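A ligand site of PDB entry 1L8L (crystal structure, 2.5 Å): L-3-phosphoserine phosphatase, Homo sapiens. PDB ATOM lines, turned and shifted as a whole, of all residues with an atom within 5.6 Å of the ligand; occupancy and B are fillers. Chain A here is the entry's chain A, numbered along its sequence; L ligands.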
ATOM      1  N   ASP A  20     -11.983  28.640   3.530  1.00  0.00           N
ATOM      2  CA  ASP A  20     -11.083  27.796   4.189  1.00  0.00           C
ATOM      3  C   ASP A  20     -10.117  28.754   4.770  1.00  0.00           C
ATOM      4  O   ASP A  20      -9.552  29.603   4.087  1.00  0.00           O
ATOM      5  CB  ASP A  20     -10.391  26.927   3.133  1.00  0.00           C
ATOM      6  CG  ASP A  20      -9.499  25.911   3.831  1.00  0.00           C
ATOM      7  OD1 ASP A  20      -8.357  26.259   4.144  1.00  0.00           O
ATOM      8  OD2 ASP A  20      -9.940  24.790   4.055  1.00  0.00           O
ATOM      9  N   VAL A  21     -10.001  28.739   5.796  1.00  0.00           N
ATOM     10  CA  VAL A  21      -8.919  29.671   6.114  1.00  0.00           C
ATOM     11  C   VAL A  21      -7.526  29.141   5.864  1.00  0.00           C
ATOM     12  O   VAL A  21      -6.809  29.695   5.037  1.00  0.00           O
ATOM     13  CB  VAL A  21      -9.070  30.123   7.576  1.00  0.00           C
ATOM     14  CG1 VAL A  21      -7.902  30.775   8.305  1.00  0.00           C
ATOM     15  CG2 VAL A  21     -10.341  30.900   7.859  1.00  0.00           C
ATOM     16  N   ASP A  22      -7.135  28.062   6.543  1.00  0.00           N
ATOM     17  CA  ASP A  22      -5.781  27.544   6.375  1.00  0.00           C
ATOM     18  C   ASP A  22      -5.462  27.144   4.941  1.00  0.00           C
ATOM     19  O   ASP A  22      -6.145  26.304   4.335  1.00  0.00           O
ATOM     20  CB  ASP A  22      -5.490  26.336   7.298  1.00  0.00           C
ATOM     21  CG  ASP A  22      -5.666  26.651   8.791  1.00  0.00           C
ATOM     22  OD1 ASP A  22      -5.454  27.817   9.217  1.00  0.00           O
ATOM     23  OD2 ASP A  22      -6.003  25.721   9.545  1.00  0.00           O
ATOM     24  N   SER A  23      -4.425  27.758   4.404  1.00  0.00           N
ATOM     25  CA  SER A  23      -3.944  27.482   3.071  1.00  0.00           C
ATOM     26  C   SER A  23      -4.798  28.066   1.974  1.00  0.00           C
ATOM     27  O   SER A  23      -4.638  27.732   0.797  1.00  0.00           O
ATOM     28  CB  SER A  23      -3.720  25.983   2.891  1.00  0.00           C
ATOM     29  OG  SER A  23      -2.572  25.570   3.619  1.00  0.00           O
ATOM     30  N   GLU A  29      -0.827  27.687   8.114  1.00  0.00           N
ATOM     31  CA  GLU A  29      -1.801  26.784   8.728  1.00  0.00           C
ATOM     32  C   GLU A  29      -1.905  27.015  10.239  1.00  0.00           C
ATOM     33  O   GLU A  29      -0.934  27.340  10.907  1.00  0.00           O
ATOM     34  CB  GLU A  29      -1.347  25.347   8.452  1.00  0.00           C
ATOM     35  CG  GLU A  29      -2.350  24.579   7.583  1.00  0.00           C
ATOM     36  CD  GLU A  29      -2.809  23.341   8.318  1.00  0.00           C
ATOM     37  OE1 GLU A  29      -2.341  23.108   9.421  1.00  0.00           O
ATOM     38  OE2 GLU A  29      -3.633  22.604   7.768  1.00  0.00           O
ATOM     39  N   ILE A  31      -2.890  25.255  12.873  1.00  0.00           N
ATOM     40  CA  ILE A  31      -2.412  24.209  13.772  1.00  0.00           C
ATOM     41  C   ILE A  31      -0.869  24.137  13.856  1.00  0.00           C
ATOM     42  O   ILE A  31      -0.300  24.208  14.953  1.00  0.00           O
ATOM     43  CB  ILE A  31      -3.031  22.842  13.338  1.00  0.00           C
ATOM     44  CG1 ILE A  31      -4.545  23.066  13.005  1.00  0.00           C
ATOM     45  CG2 ILE A  31      -2.841  21.790  14.441  1.00  0.00           C
ATOM     46  CD1 ILE A  31      -5.365  21.833  12.584  1.00  0.00           C
ATOM     47  N   ILE A 108     -14.509  28.932   7.128  1.00  0.00           N
ATOM     48  CA  ILE A 108     -14.679  27.571   7.654  1.00  0.00           C
ATOM     49  C   ILE A 108     -13.376  26.821   7.897  1.00  0.00           C
ATOM     50  O   ILE A 108     -12.582  26.646   6.989  1.00  0.00           O
ATOM     51  CB  ILE A 108     -15.443  26.662   6.658  1.00  0.00           C
ATOM     52  CG1 ILE A 108     -16.672  27.405   6.110  1.00  0.00           C
ATOM     53  CG2 ILE A 108     -15.956  25.440   7.402  1.00  0.00           C
ATOM     54  CD1 ILE A 108     -17.419  26.654   5.044  1.00  0.00           C
ATOM     55  N   SER A 109     -13.122  26.426   9.141  1.00  0.00           N
ATOM     56  CA  SER A 109     -11.802  25.799   9.425  1.00  0.00           C
ATOM     57  C   SER A 109     -11.809  24.581  10.408  1.00  0.00           C
ATOM     58  O   SER A 109     -12.654  24.469  11.283  1.00  0.00           O
ATOM     59  CB  SER A 109     -10.865  26.878   9.958  1.00  0.00           C
ATOM     60  OG  SER A 109      -9.510  26.446   9.834  1.00  0.00           O
ATOM     61  N   GLY A 110     -10.774  23.755  10.260  1.00  0.00           N
ATOM     62  CA  GLY A 110     -10.553  22.672  11.181  1.00  0.00           C
ATOM     63  C   GLY A 110      -9.657  23.255  12.246  1.00  0.00           C
ATOM     64  O   GLY A 110      -9.404  22.639  13.267  1.00  0.00           O
ATOM     65  N   GLY A 111      -9.192  24.472  11.976  1.00  0.00           N
ATOM     66  CA  GLY A 111      -8.327  25.200  12.892  1.00  0.00           C
ATOM     67  C   GLY A 111      -9.033  25.575  14.179  1.00  0.00           C
ATOM     68  O   GLY A 111      -9.870  24.827  14.657  1.00  0.00           O
ATOM     69  N   LYS A 158     -16.846  19.380   7.289  1.00  0.00           N
ATOM     70  CA  LYS A 158     -16.696  20.669   6.627  1.00  0.00           C
ATOM     71  C   LYS A 158     -17.937  21.008   5.792  1.00  0.00           C
ATOM     72  O   LYS A 158     -18.286  22.176   5.618  1.00  0.00           O
ATOM     73  CB  LYS A 158     -15.468  20.650   5.719  1.00  0.00           C
ATOM     74  CG  LYS A 158     -15.158  22.000   5.104  1.00  0.00           C
ATOM     75  CD  LYS A 158     -14.062  22.746   5.850  1.00  0.00           C
ATOM     76  CE  LYS A 158     -12.716  22.078   5.712  1.00  0.00           C
ATOM     77  NZ  LYS A 158     -11.576  22.904   6.215  1.00  0.00           N
ATOM     78  N   ASP A 179      -8.403  24.923  -0.610  1.00  0.00           N
ATOM     79  CA  ASP A 179      -7.187  24.279  -1.109  1.00  0.00           C
ATOM     80  C   ASP A 179      -6.971  22.765  -1.080  1.00  0.00           C
ATOM     81  O   ASP A 179      -6.144  22.257  -1.830  1.00  0.00           O
ATOM     82  CB  ASP A 179      -6.087  24.889  -0.245  1.00  0.00           C
ATOM     83  CG  ASP A 179      -5.824  24.076   1.009  1.00  0.00           C
ATOM     84  OD1 ASP A 179      -6.632  24.199   1.964  1.00  0.00           O
ATOM     85  OD2 ASP A 179      -4.825  23.320   1.028  1.00  0.00           O
ATOM     86  N   GLY A 180      -7.673  22.061  -0.211  1.00  0.00           N
ATOM     87  CA  GLY A 180      -7.471  20.619  -0.141  1.00  0.00           C
ATOM     88  C   GLY A 180      -8.722  19.851  -0.529  1.00  0.00           C
ATOM     89  O   GLY A 180      -9.762  20.453  -0.718  1.00  0.00           O
ATOM     90  N   ALA A 181      -8.629  18.530  -0.626  1.00  0.00           N
ATOM     91  CA  ALA A 181      -9.785  17.733  -1.012  1.00  0.00           C
ATOM     92  C   ALA A 181     -10.916  17.726   0.011  1.00  0.00           C
ATOM     93  O   ALA A 181     -11.978  17.159  -0.248  1.00  0.00           O
ATOM     94  CB  ALA A 181      -9.368  16.313  -1.323  1.00  0.00           C
ATOM     95  N   THR A 182     -10.693  18.335   1.173  1.00  0.00           N
ATOM     96  CA  THR A 182     -11.733  18.378   2.199  1.00  0.00           C
ATOM     97  C   THR A 182     -12.673  19.537   1.867  1.00  0.00           C
ATOM     98  O   THR A 182     -13.884  19.471   2.065  1.00  0.00           O
ATOM     99  CB  THR A 182     -11.136  18.607   3.600  1.00  0.00           C
ATOM    100  OG1 THR A 182     -10.212  17.548   3.885  1.00  0.00           O
ATOM    101  CG2 THR A 182     -12.215  18.580   4.638  1.00  0.00           C
ATOM    102  N   ASP A 183     -12.070  20.604   1.352  1.00  0.00           N
ATOM    103  CA  ASP A 183     -12.773  21.797   0.929  1.00  0.00           C
ATOM    104  C   ASP A 183     -13.582  21.399  -0.297  1.00  0.00           C
ATOM    105  O   ASP A 183     -14.745  21.766  -0.426  1.00  0.00           O
ATOM    106  CB  ASP A 183     -11.769  22.878   0.551  1.00  0.00           C
ATOM    107  CG  ASP A 183     -10.971  23.361   1.737  1.00  0.00           C
ATOM    108  OD1 ASP A 183      -9.823  23.801   1.553  1.00  0.00           O
ATOM    109  OD2 ASP A 183     -11.495  23.302   2.868  1.00  0.00           O
HETATM  110  C1  LIG L   1      -8.094  21.393   5.206  1.00  0.00           C
HETATM  111  N1  LIG L   1      -9.432  20.801   5.440  1.00  0.00           N
HETATM  112  C2  LIG L   1      -7.473  20.946   3.841  1.00  0.00           C
HETATM  113  O1  LIG L   1      -6.570  21.580   3.301  1.00  0.00           O
HETATM  114  O2  LIG L   1      -7.991  19.783   3.309  1.00  0.00           O
HETATM  115  C3  LIG L   1      -8.256  22.947   5.428  1.00  0.00           C
HETATM  116  P1  LIG L   1      -8.036  23.459   7.120  1.00  0.00           P
HETATM  117  O3  LIG L   1      -9.287  22.826   7.921  1.00  0.00           O
HETATM  118  O4  LIG L   1      -6.662  22.858   7.744  1.00  0.00           O
HETATM  119  O5  LIG L   1      -8.171  25.053   7.331  1.00  0.00           O
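The side-chain amino group (NZ) of Lys 158 is in salt-bridge range of an oxygen (O3) of the ligand (2.9 Å). The backbone NH of Gly 110 sits at hydrogen-bond distance from an oxygen (O3) of the ligand, 2.9 Å away. O1 of the ligand lies close to OD1 of Asp 179 (2.9 Å). An oxygen (O5) of the ligand sits close to the backbone NH (N) of Asp 22. O4 of the ligand lies close to OE2 of Glu 29, at 3.0 Å. An oxygen (O5) of the ligand sits at hydrogen-bond distance from the side-chain hydroxyl of Ser 109 (3.2 Å). An oxygen (O2) of the ligand sits at hydrogen-bond distance from the side-chain hydroxyl of Thr 182 (3.2 Å).
NZ of Lys 158 lies within salt-bridge range of OD2 of Asp 20 (3.3 Å). N of Asp 22 lies close to OD1 of Asp 20. OD2 of Asp 183 sits close to OD2 of Asp 20 (2.5 Å). The side-chain amino group of Lys 158 is in salt-bridge range of the side-chain carboxylate of Asp 183, at 3.4 Å. The side-chain carboxylate (OD1) of Asp 183 is in hydrogen-bond range of the backbone NH (N) of Asp 179, 2.8 Å away. The side-chain hydroxyl (OG) of Ser 109 lies within hydrogen-bond range of the backbone NH (N) of Gly 111 (2.9 Å). The side-chain carboxylate (OD1) of Asp 183 is in hydrogen-bond range of the backbone NH (N) of Gly 180 (3.3 Å).
OD1 of Asp 20 sits close to O5 of the ligand (3.4 Å). Gly 180 touches the ligand. Of the 16 residues printed, 9 come within 4 Å of the ligand. The nearest printed residue that does not touch the ligand is Asp 183 (4.1 Å).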
